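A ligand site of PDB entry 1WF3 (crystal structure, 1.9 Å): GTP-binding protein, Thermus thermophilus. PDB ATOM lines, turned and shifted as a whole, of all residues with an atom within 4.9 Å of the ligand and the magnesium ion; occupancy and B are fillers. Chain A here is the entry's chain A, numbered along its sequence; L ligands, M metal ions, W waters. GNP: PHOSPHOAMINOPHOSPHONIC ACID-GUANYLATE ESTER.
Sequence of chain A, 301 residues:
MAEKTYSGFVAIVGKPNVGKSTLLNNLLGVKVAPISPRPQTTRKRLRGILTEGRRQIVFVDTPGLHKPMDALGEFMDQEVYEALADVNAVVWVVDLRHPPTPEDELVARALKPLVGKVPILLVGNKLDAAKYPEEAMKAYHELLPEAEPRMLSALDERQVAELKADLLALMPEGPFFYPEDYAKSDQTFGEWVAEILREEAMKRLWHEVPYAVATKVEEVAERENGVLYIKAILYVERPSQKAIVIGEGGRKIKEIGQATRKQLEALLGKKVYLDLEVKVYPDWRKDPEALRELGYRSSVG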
ATOM      1  N   LYS A  15     -27.006  11.404   6.810  1.00  0.00           N
ATOM      2  CA  LYS A  15     -26.325  12.304   5.880  1.00  0.00           C
ATOM      3  C   LYS A  15     -25.849  11.472   4.681  1.00  0.00           C
ATOM      4  O   LYS A  15     -25.948  10.242   4.682  1.00  0.00           O
ATOM      5  CB  LYS A  15     -25.127  12.996   6.565  1.00  0.00           C
ATOM      6  CG  LYS A  15     -23.913  12.097   6.779  1.00  0.00           C
ATOM      7  CD  LYS A  15     -22.730  12.892   7.313  1.00  0.00           C
ATOM      8  CE  LYS A  15     -21.472  12.039   7.309  1.00  0.00           C
ATOM      9  NZ  LYS A  15     -21.090  11.630   5.911  1.00  0.00           N
ATOM     10  N   PRO A  16     -25.288  12.126   3.650  1.00  0.00           N
ATOM     11  CA  PRO A  16     -24.841  11.328   2.502  1.00  0.00           C
ATOM     12  C   PRO A  16     -23.632  10.435   2.774  1.00  0.00           C
ATOM     13  O   PRO A  16     -22.838  10.663   3.710  1.00  0.00           O
ATOM     14  CB  PRO A  16     -24.502  12.402   1.450  1.00  0.00           C
ATOM     15  CG  PRO A  16     -25.254  13.640   1.899  1.00  0.00           C
ATOM     16  CD  PRO A  16     -25.101  13.562   3.411  1.00  0.00           C
ATOM     17  N   ASN A  17     -23.528   9.378   1.977  1.00  0.00           N
ATOM     18  CA  ASN A  17     -22.369   8.483   2.004  1.00  0.00           C
ATOM     19  C   ASN A  17     -22.171   7.597   3.228  1.00  0.00           C
ATOM     20  O   ASN A  17     -21.084   7.041   3.400  1.00  0.00           O
ATOM     21  CB  ASN A  17     -21.103   9.340   1.775  1.00  0.00           C
ATOM     22  CG  ASN A  17     -20.281   8.867   0.579  1.00  0.00           C
ATOM     23  OD1 ASN A  17     -20.648   7.925  -0.115  1.00  0.00           O
ATOM     24  ND2 ASN A  17     -19.158   9.549   0.335  1.00  0.00           N
ATOM     25  N   VAL A  18     -23.199   7.433   4.060  1.00  0.00           N
ATOM     26  CA  VAL A  18     -23.066   6.589   5.254  1.00  0.00           C
ATOM     27  C   VAL A  18     -23.383   5.117   5.016  1.00  0.00           C
ATOM     28  O   VAL A  18     -23.066   4.270   5.839  1.00  0.00           O
ATOM     29  CB  VAL A  18     -23.954   7.117   6.401  1.00  0.00           C
ATOM     30  CG1 VAL A  18     -23.485   8.518   6.800  1.00  0.00           C
ATOM     31  CG2 VAL A  18     -25.435   7.124   5.975  1.00  0.00           C
ATOM     32  N   GLY A  19     -24.040   4.833   3.879  1.00  0.00           N
ATOM     33  CA  GLY A  19     -24.363   3.457   3.539  1.00  0.00           C
ATOM     34  C   GLY A  19     -25.839   3.092   3.584  1.00  0.00           C
ATOM     35  O   GLY A  19     -26.179   1.915   3.725  1.00  0.00           O
ATOM     36  N   LYS A  20     -26.709   4.087   3.493  1.00  0.00           N
ATOM     37  CA  LYS A  20     -28.154   3.836   3.534  1.00  0.00           C
ATOM     38  C   LYS A  20     -28.635   2.909   2.425  1.00  0.00           C
ATOM     39  O   LYS A  20     -29.366   1.965   2.678  1.00  0.00           O
ATOM     40  CB  LYS A  20     -28.920   5.161   3.470  1.00  0.00           C
ATOM     41  CG  LYS A  20     -28.619   6.078   4.666  1.00  0.00           C
ATOM     42  CD  LYS A  20     -29.447   7.352   4.660  1.00  0.00           C
ATOM     43  CE  LYS A  20     -29.210   8.172   3.398  1.00  0.00           C
ATOM     44  NZ  LYS A  20     -27.759   8.554   3.203  1.00  0.00           N
ATOM     45  N   SER A  21     -28.224   3.189   1.191  1.00  0.00           N
ATOM     46  CA  SER A  21     -28.651   2.347   0.085  1.00  0.00           C
ATOM     47  C   SER A  21     -28.001   0.963   0.147  1.00  0.00           C
ATOM     48  O   SER A  21     -28.599  -0.037  -0.249  1.00  0.00           O
ATOM     49  CB  SER A  21     -28.316   3.018  -1.241  1.00  0.00           C
ATOM     50  OG  SER A  21     -29.027   4.239  -1.310  1.00  0.00           O
ATOM     51  N   THR A  22     -26.756   0.908   0.613  1.00  0.00           N
ATOM     52  CA  THR A  22     -26.068  -0.363   0.763  1.00  0.00           C
ATOM     53  C   THR A  22     -26.839  -1.191   1.780  1.00  0.00           C
ATOM     54  O   THR A  22     -27.051  -2.406   1.597  1.00  0.00           O
ATOM     55  CB  THR A  22     -24.625  -0.154   1.270  1.00  0.00           C
ATOM     56  OG1 THR A  22     -23.883   0.589   0.298  1.00  0.00           O
ATOM     57  CG2 THR A  22     -23.955  -1.513   1.539  1.00  0.00           C
ATOM     58  N   PRO A  34     -29.028   2.384  -6.108  1.00  0.00           N
ATOM     59  CA  PRO A  34     -27.697   2.758  -6.595  1.00  0.00           C
ATOM     60  C   PRO A  34     -26.797   3.031  -5.397  1.00  0.00           C
ATOM     61  O   PRO A  34     -27.253   3.513  -4.349  1.00  0.00           O
ATOM     62  CB  PRO A  34     -27.962   4.011  -7.419  1.00  0.00           C
ATOM     63  CG  PRO A  34     -29.112   4.650  -6.669  1.00  0.00           C
ATOM     64  CD  PRO A  34     -30.004   3.459  -6.361  1.00  0.00           C
ATOM     65  N   ILE A  35     -25.521   2.724  -5.566  1.00  0.00           N
ATOM     66  CA  ILE A  35     -24.531   2.907  -4.532  1.00  0.00           C
ATOM     67  C   ILE A  35     -23.255   3.496  -5.126  1.00  0.00           C
ATOM     68  O   ILE A  35     -22.830   3.095  -6.222  1.00  0.00           O
ATOM     69  CB  ILE A  35     -24.215   1.561  -3.863  1.00  0.00           C
ATOM     70  CG1 ILE A  35     -25.413   1.119  -3.025  1.00  0.00           C
ATOM     71  CG2 ILE A  35     -22.949   1.672  -3.031  1.00  0.00           C
ATOM     72  CD1 ILE A  35     -25.202  -0.202  -2.360  1.00  0.00           C
ATOM     73  N   SER A  36     -22.646   4.448  -4.433  1.00  0.00           N
ATOM     74  CA  SER A  36     -21.397   5.026  -4.933  1.00  0.00           C
ATOM     75  C   SER A  36     -20.613   5.663  -3.811  1.00  0.00           C
ATOM     76  O   SER A  36     -21.149   5.908  -2.723  1.00  0.00           O
ATOM     77  CB  SER A  36     -21.666   6.055  -6.032  1.00  0.00           C
ATOM     78  OG  SER A  36     -21.634   7.406  -5.561  1.00  0.00           O
ATOM     79  N   PRO A  37     -19.326   5.950  -4.049  1.00  0.00           N
ATOM     80  CA  PRO A  37     -18.510   6.564  -3.013  1.00  0.00           C
ATOM     81  C   PRO A  37     -18.658   8.089  -3.006  1.00  0.00           C
ATOM     82  O   PRO A  37     -18.017   8.771  -2.220  1.00  0.00           O
ATOM     83  CB  PRO A  37     -17.108   6.086  -3.369  1.00  0.00           C
ATOM     84  CG  PRO A  37     -17.150   6.054  -4.849  1.00  0.00           C
ATOM     85  CD  PRO A  37     -18.498   5.438  -5.152  1.00  0.00           C
ATOM     86  N   ARG A  38     -19.502   8.600  -3.895  1.00  0.00           N
ATOM     87  CA  ARG A  38     -19.734  10.042  -3.976  1.00  0.00           C
ATOM     88  C   ARG A  38     -20.851  10.466  -3.005  1.00  0.00           C
ATOM     89  O   ARG A  38     -21.882   9.828  -2.937  1.00  0.00           O
ATOM     90  CB  ARG A  38     -20.155  10.419  -5.397  1.00  0.00           C
ATOM     91  CG  ARG A  38     -19.149  10.000  -6.455  1.00  0.00           C
ATOM     92  CD  ARG A  38     -17.936  10.910  -6.498  1.00  0.00           C
ATOM     93  NE  ARG A  38     -17.046  10.490  -7.567  1.00  0.00           N
ATOM     94  CZ  ARG A  38     -16.051   9.623  -7.426  1.00  0.00           C
ATOM     95  NH1 ARG A  38     -15.789   9.066  -6.250  1.00  0.00           N
ATOM     96  NH2 ARG A  38     -15.337   9.268  -8.483  1.00  0.00           N
ATOM     97  N   PRO A  39     -20.628  11.562  -2.266  1.00  0.00           N
ATOM     98  CA  PRO A  39     -21.510  12.184  -1.270  1.00  0.00           C
ATOM     99  C   PRO A  39     -22.862  12.740  -1.710  1.00  0.00           C
ATOM    100  O   PRO A  39     -23.305  13.732  -1.148  1.00  0.00           O
ATOM    101  CB  PRO A  39     -20.653  13.315  -0.679  1.00  0.00           C
ATOM    102  CG  PRO A  39     -19.246  12.949  -1.057  1.00  0.00           C
ATOM    103  CD  PRO A  39     -19.362  12.307  -2.382  1.00  0.00           C
ATOM    104  N   GLN A  40     -23.487  12.145  -2.723  1.00  0.00           N
ATOM    105  CA  GLN A  40     -24.816  12.567  -3.156  1.00  0.00           C
ATOM    106  C   GLN A  40     -25.309  11.609  -4.243  1.00  0.00           C
ATOM    107  O   GLN A  40     -25.488  11.987  -5.390  1.00  0.00           O
ATOM    108  CB  GLN A  40     -24.800  13.988  -3.722  1.00  0.00           C
ATOM    109  CG  GLN A  40     -26.213  14.593  -3.804  1.00  0.00           C
ATOM    110  CD  GLN A  40     -26.212  16.013  -4.344  1.00  0.00           C
ATOM    111  OE1 GLN A  40     -26.305  16.224  -5.551  1.00  0.00           O
ATOM    112  NE2 GLN A  40     -26.080  16.994  -3.455  1.00  0.00           N
ATOM    113  N   THR A  41     -25.531  10.366  -3.861  1.00  0.00           N
ATOM    114  CA  THR A  41     -25.966   9.367  -4.831  1.00  0.00           C
ATOM    115  C   THR A  41     -27.493   9.292  -4.967  1.00  0.00           C
ATOM    116  O   THR A  41     -28.033   9.571  -6.032  1.00  0.00           O
ATOM    117  CB  THR A  41     -25.360   8.000  -4.465  1.00  0.00           C
ATOM    118  OG1 THR A  41     -23.927   8.158  -4.391  1.00  0.00           O
ATOM    119  CG2 THR A  41     -25.676   6.932  -5.520  1.00  0.00           C
ATOM    120  N   THR A  42     -28.184   8.947  -3.882  1.00  0.00           N
ATOM    121  CA  THR A  42     -29.646   8.837  -3.923  1.00  0.00           C
ATOM    122  C   THR A  42     -30.269  10.228  -3.998  1.00  0.00           C
ATOM    123  O   THR A  42     -29.862  11.112  -3.273  1.00  0.00           O
ATOM    124  CB  THR A  42     -30.158   8.115  -2.675  1.00  0.00           C
ATOM    125  OG1 THR A  42     -29.600   6.791  -2.668  1.00  0.00           O
ATOM    126  CG2 THR A  42     -31.696   8.016  -2.670  1.00  0.00           C
ATOM    127  N   ASP A  61     -35.777   4.217   1.283  1.00  0.00           N
ATOM    128  CA  ASP A  61     -34.411   4.742   1.184  1.00  0.00           C
ATOM    129  C   ASP A  61     -34.613   6.223   0.871  1.00  0.00           C
ATOM    130  O   ASP A  61     -35.590   6.608   0.199  1.00  0.00           O
ATOM    131  CB  ASP A  61     -33.666   4.014   0.059  1.00  0.00           C
ATOM    132  CG  ASP A  61     -32.190   4.404  -0.023  1.00  0.00           C
ATOM    133  OD1 ASP A  61     -31.646   4.990   0.952  1.00  0.00           O
ATOM    134  OD2 ASP A  61     -31.551   4.101  -1.065  1.00  0.00           O
ATOM    135  N   THR A  62     -33.716   7.076   1.349  1.00  0.00           N
ATOM    136  CA  THR A  62     -33.854   8.494   1.143  1.00  0.00           C
ATOM    137  C   THR A  62     -32.549   9.144   0.773  1.00  0.00           C
ATOM    138  O   THR A  62     -31.469   8.560   0.974  1.00  0.00           O
ATOM    139  CB  THR A  62     -34.364   9.188   2.454  1.00  0.00           C
ATOM    140  OG1 THR A  62     -33.397   9.013   3.500  1.00  0.00           O
ATOM    141  CG2 THR A  62     -35.723   8.578   2.921  1.00  0.00           C
ATOM    142  N   PRO A  63     -32.615  10.353   0.209  1.00  0.00           N
ATOM    143  CA  PRO A  63     -31.413  11.094  -0.179  1.00  0.00           C
ATOM    144  C   PRO A  63     -30.716  11.494   1.123  1.00  0.00           C
ATOM    145  O   PRO A  63     -31.376  11.685   2.159  1.00  0.00           O
ATOM    146  CB  PRO A  63     -31.968  12.351  -0.885  1.00  0.00           C
ATOM    147  CG  PRO A  63     -33.339  11.948  -1.335  1.00  0.00           C
ATOM    148  CD  PRO A  63     -33.836  11.065  -0.212  1.00  0.00           C
ATOM    149  N   GLY A  64     -29.392  11.624   1.081  1.00  0.00           N
ATOM    150  CA  GLY A  64     -28.665  12.056   2.264  1.00  0.00           C
ATOM    151  C   GLY A  64     -29.070  13.478   2.636  1.00  0.00           C
ATOM    152  O   GLY A  64     -29.124  14.368   1.780  1.00  0.00           O
ATOM    153  N   ASN A 125     -22.695   2.339  10.950  1.00  0.00           N
ATOM    154  CA  ASN A 125     -22.270   1.497   9.853  1.00  0.00           C
ATOM    155  C   ASN A 125     -20.757   1.567   9.580  1.00  0.00           C
ATOM    156  O   ASN A 125     -20.068   2.440  10.101  1.00  0.00           O
ATOM    157  CB  ASN A 125     -23.042   1.915   8.587  1.00  0.00           C
ATOM    158  CG  ASN A 125     -22.885   0.922   7.460  1.00  0.00           C
ATOM    159  OD1 ASN A 125     -22.791  -0.284   7.685  1.00  0.00           O
ATOM    160  ND2 ASN A 125     -22.903   1.430   6.222  1.00  0.00           N
ATOM    161  N   LYS A 126     -20.274   0.650   8.751  1.00  0.00           N
ATOM    162  CA  LYS A 126     -18.863   0.546   8.361  1.00  0.00           C
ATOM    163  C   LYS A 126     -17.969   0.170   9.536  1.00  0.00           C
ATOM    164  O   LYS A 126     -16.804   0.618   9.635  1.00  0.00           O
ATOM    165  CB  LYS A 126     -18.380   1.840   7.726  1.00  0.00           C
ATOM    166  CG  LYS A 126     -19.270   2.332   6.570  1.00  0.00           C
ATOM    167  CD  LYS A 126     -18.675   3.557   5.883  1.00  0.00           C
ATOM    168  CE  LYS A 126     -19.637   4.130   4.837  1.00  0.00           C
ATOM    169  NZ  LYS A 126     -19.039   5.305   4.153  1.00  0.00           N
ATOM    170  N   ASP A 128     -16.483  -2.416   9.977  1.00  0.00           N
ATOM    171  CA  ASP A 128     -15.330  -3.093   9.391  1.00  0.00           C
ATOM    172  C   ASP A 128     -14.138  -2.187   9.082  1.00  0.00           C
ATOM    173  O   ASP A 128     -12.990  -2.651   9.056  1.00  0.00           O
ATOM    174  CB  ASP A 128     -15.753  -3.757   8.087  1.00  0.00           C
ATOM    175  CG  ASP A 128     -16.204  -2.741   7.050  1.00  0.00           C
ATOM    176  OD1 ASP A 128     -17.253  -2.114   7.283  1.00  0.00           O
ATOM    177  OD2 ASP A 128     -15.517  -2.554   6.031  1.00  0.00           O
ATOM    178  N   ALA A 129     -14.394  -0.916   8.843  1.00  0.00           N
ATOM    179  CA  ALA A 129     -13.332   0.016   8.482  1.00  0.00           C
ATOM    180  C   ALA A 129     -13.105   1.145   9.465  1.00  0.00           C
ATOM    181  O   ALA A 129     -12.320   2.044   9.198  1.00  0.00           O
ATOM    182  CB  ALA A 129     -13.629   0.618   7.099  1.00  0.00           C
ATOM    183  N   SER A 153     -21.782  -3.594   9.962  1.00  0.00           N
ATOM    184  CA  SER A 153     -21.319  -3.275   8.614  1.00  0.00           C
ATOM    185  C   SER A 153     -22.501  -3.740   7.785  1.00  0.00           C
ATOM    186  O   SER A 153     -22.992  -4.853   7.986  1.00  0.00           O
ATOM    187  CB  SER A 153     -20.096  -4.087   8.201  1.00  0.00           C
ATOM    188  OG  SER A 153     -19.898  -3.980   6.792  1.00  0.00           O
ATOM    189  N   ALA A 154     -22.958  -2.890   6.874  1.00  0.00           N
ATOM    190  CA  ALA A 154     -24.089  -3.229   6.033  1.00  0.00           C
ATOM    191  C   ALA A 154     -23.734  -4.412   5.143  1.00  0.00           C
ATOM    192  O   ALA A 154     -24.605  -5.052   4.560  1.00  0.00           O
ATOM    193  CB  ALA A 154     -24.491  -2.002   5.170  1.00  0.00           C
ATOM    194  N   LEU A 155     -22.445  -4.729   5.090  1.00  0.00           N
ATOM    195  CA  LEU A 155     -21.954  -5.843   4.278  1.00  0.00           C
ATOM    196  C   LEU A 155     -21.888  -7.169   5.039  1.00  0.00           C
ATOM    197  O   LEU A 155     -21.591  -8.211   4.455  1.00  0.00           O
ATOM    198  CB  LEU A 155     -20.552  -5.496   3.757  1.00  0.00           C
ATOM    199  CG  LEU A 155     -20.521  -4.191   2.950  1.00  0.00           C
ATOM    200  CD1 LEU A 155     -19.086  -3.842   2.591  1.00  0.00           C
ATOM    201  CD2 LEU A 155     -21.369  -4.357   1.694  1.00  0.00           C
HETATM  202  PG  GNP L   1     -26.475   8.914  -0.403  1.00  0.00           P
HETATM  203  O1G GNP L   1     -25.747   9.971  -1.162  1.00  0.00           O
HETATM  204  O2G GNP L   1     -27.396   8.142  -1.302  1.00  0.00           O
HETATM  205  O3G GNP L   1     -27.206   9.473   0.764  1.00  0.00           O
HETATM  206  N3B GNP L   1     -25.323   7.774   0.123  1.00  0.00           N
HETATM  207  PB  GNP L   1     -25.710   6.432   1.010  1.00  0.00           P
HETATM  208  O1B GNP L   1     -25.860   6.682   2.455  1.00  0.00           O
HETATM  209  O2B GNP L   1     -26.875   5.696   0.425  1.00  0.00           O
HETATM  210  O3A GNP L   1     -24.384   5.528   0.847  1.00  0.00           O
HETATM  211  PA  GNP L   1     -24.143   4.281  -0.139  1.00  0.00           P
HETATM  212  O1A GNP L   1     -24.972   3.102   0.166  1.00  0.00           O
HETATM  213  O2A GNP L   1     -24.224   4.843  -1.551  1.00  0.00           O
HETATM  214  O5' GNP L   1     -22.658   3.982   0.333  1.00  0.00           O
HETATM  215  C5' GNP L   1     -21.630   4.987   0.216  1.00  0.00           C
HETATM  216  C4' GNP L   1     -20.279   4.320   0.196  1.00  0.00           C
HETATM  217  O4' GNP L   1     -20.059   3.604   1.471  1.00  0.00           O
HETATM  218  C3' GNP L   1     -20.097   3.255  -0.909  1.00  0.00           C
HETATM  219  O3' GNP L   1     -18.734   3.373  -1.429  1.00  0.00           O
HETATM  220  C2' GNP L   1     -20.303   1.964  -0.194  1.00  0.00           C
HETATM  221  O2' GNP L   1     -19.705   0.819  -0.811  1.00  0.00           O
HETATM  222  C1' GNP L   1     -19.700   2.233   1.199  1.00  0.00           C
HETATM  223  N9  GNP L   1     -20.211   1.398   2.275  1.00  0.00           N
HETATM  224  C8  GNP L   1     -21.518   1.153   2.648  1.00  0.00           C
HETATM  225  N7  GNP L   1     -21.668   0.346   3.669  1.00  0.00           N
HETATM  226  C5  GNP L   1     -20.342   0.029   3.995  1.00  0.00           C
HETATM  227  C6  GNP L   1     -19.837  -0.827   5.032  1.00  0.00           C
HETATM  228  O6  GNP L   1     -20.440  -1.481   5.879  1.00  0.00           O
HETATM  229  N1  GNP L   1     -18.384  -0.882   5.037  1.00  0.00           N
HETATM  230  C2  GNP L   1     -17.574  -0.203   4.156  1.00  0.00           C
HETATM  231  N2  GNP L   1     -16.242  -0.375   4.309  1.00  0.00           N
HETATM  232  N3  GNP L   1     -18.051   0.601   3.170  1.00  0.00           N
HETATM  233  C4  GNP L   1     -19.447   0.666   3.155  1.00  0.00           C
HETATM  234 MG    MG M   1     -28.150   6.211  -1.155  1.00  0.00          MG
HETATM  235  O   HOH W   1     -23.287   7.570  -1.787  1.00  0.00           O
HETATM  236  O   HOH W   2     -27.802  11.701  -1.536  1.00  0.00           O
HETATM  237  O   HOH W   3     -26.668   5.460  -2.615  1.00  0.00           O
HETATM  238  O   HOH W   4     -18.790   2.352  -4.030  1.00  0.00           O
HETATM  239  O   HOH W   5     -16.967   4.073   2.773  1.00  0.00           O
HETATM  240  O   HOH W   6     -29.701   6.681   0.326  1.00  0.00           O
HETATM  241  O   HOH W   7     -16.706   4.292   0.052  1.00  0.00           O
HETATM  242  O   HOH W   8     -21.715  -0.988  -0.916  1.00  0.00           O
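Of the 28 residues printed, 2 come within 4 Å of the magnesium ion.
The magnesium ion is bound by O2G of the ligand (2.1 Å), O2B of the ligand (2.1 Å), OG of Ser 21 (2.2 Å), OG1 of Thr 42 (2.2 Å), water W6 (2.2 Å) and water W3 (2.2 Å).
An oxygen (O1A) of the ligand lies within hydrogen-bond range of the backbone NH (N) of Ser 21 (3.4 Å).
O2G of the ligand lies close to N of Thr 42, at 2.8 Å.
An oxygen (O1B) of the ligand is in hydrogen-bond range of the backbone NH of Lys 20.
O3G of the ligand lies within salt-bridge range of NZ of Lys 20, at 2.7 Å.
O6 of the ligand lies within hydrogen-bond range of OG of Ser 153 (2.7 Å).
The backbone NH (N) of Thr 41 sits at hydrogen-bond distance from an oxygen (O1G) of the ligand.
The backbone NH of Thr 22 sits at hydrogen-bond distance from an oxygen (O1A) of the ligand, at 2.9 Å.
O1A of the ligand is in hydrogen-bond range of OG1 of Thr 22.
A nitrogen (N1) of the ligand sits at hydrogen-bond distance from the side-chain carboxylate (OD1) of Asp 128 (2.8 Å).
N of Gly 19 sits at hydrogen-bond distance from O1B of the ligand.
A nitrogen (N7) of the ligand sits at hydrogen-bond distance from the side-chain amide nitrogen of Asn 125.
O6 of the ligand sits at hydrogen-bond distance from N of Ala 154, at 3.1 Å.
N of Gly 64 is in hydrogen-bond range of O3G of the ligand (3.1 Å).
O2A of the ligand sits at hydrogen-bond distance from N of Ser 36, 3.3 Å away.
An oxygen (O1B) of the ligand sits at hydrogen-bond distance from the backbone NH (N) of Val 18, at 3.2 Å.
NZ of Lys 126 is in hydrogen-bond range of O4' of the ligand (3.3 Å).
The side-chain hydroxyl (OG) of Ser 21 lies close to the side-chain carboxylate (OD2) of Asp 61 (2.5 Å).
The side-chain amino group (NZ) of Lys 20 is in hydrogen-bond range of the backbone carbonyl oxygen (O) of Lys 15, 2.9 Å away.
OG of Ser 153 lies within hydrogen-bond range of OD1 of Asp 128 (3.3 Å).
The side-chain hydroxyl (OG) of Ser 36 lies within hydrogen-bond range of the side-chain hydroxyl (OG1) of Thr 41.
OG1 of Thr 41 sits at hydrogen-bond distance from O of Arg 38 (3.0 Å).
OD1 of Asn 125 lies within hydrogen-bond range of N of Ala 154.
The side-chain amide nitrogen of Asn 125 lies within hydrogen-bond range of the backbone carbonyl oxygen of Val 18, 2.9 Å away.
The side-chain amide nitrogen of Asn 17 lies within hydrogen-bond range of the backbone carbonyl oxygen of Pro 37 (2.9 Å).
The backbone NH (N) of Asn 17 sits close to a nitrogen (N3B) of the ligand, at 3.0 Å.
Merely in contact with the ligand: Pro 16, Ile 35, Pro 37, Gln 40, Ala 129 and Leu 155.
Hydrophobic or aromatic side chains that line the ligand: Pro 16, Val 18, Ile 35, Pro 37, Ala 129, Ala 154 and Leu 155.
Within 4 Å of the ligand: Pro 16, Asn 17, Val 18, Gly 19, Lys 20, Ser 21, Thr 22, Ile 35, Ser 36, Pro 37, Gln 40, Thr 41, Thr 42, Gly 64, Asn 125, Lys 126, Asp 128, Ala 129, Ser 153, Ala 154 and Leu 155.
The nearest printed residue that does not touch the ligand is Pro 39 (4.04 Å).
Water W3 lies within hydrogen-bond range of O of Pro 34 and O2A of the ligand.
Water W6 lies within hydrogen-bond range of OD1 of Asp 61 and O of Thr 62.
Water W8 bridges O2' of the ligand (2.7 Å) and OG1 of Thr 22 (2.9 Å).
Water W2 lies within hydrogen-bond range of O1G of the ligand (2.7 Å), O of Thr 42 (2.8 Å) and N of Gly 64 (3.1 Å).
Water W5 lies within hydrogen-bond range of the side-chain amino group of Lys 126 (2.8 Å) and an oxygen (O4') of the ligand (3.4 Å).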
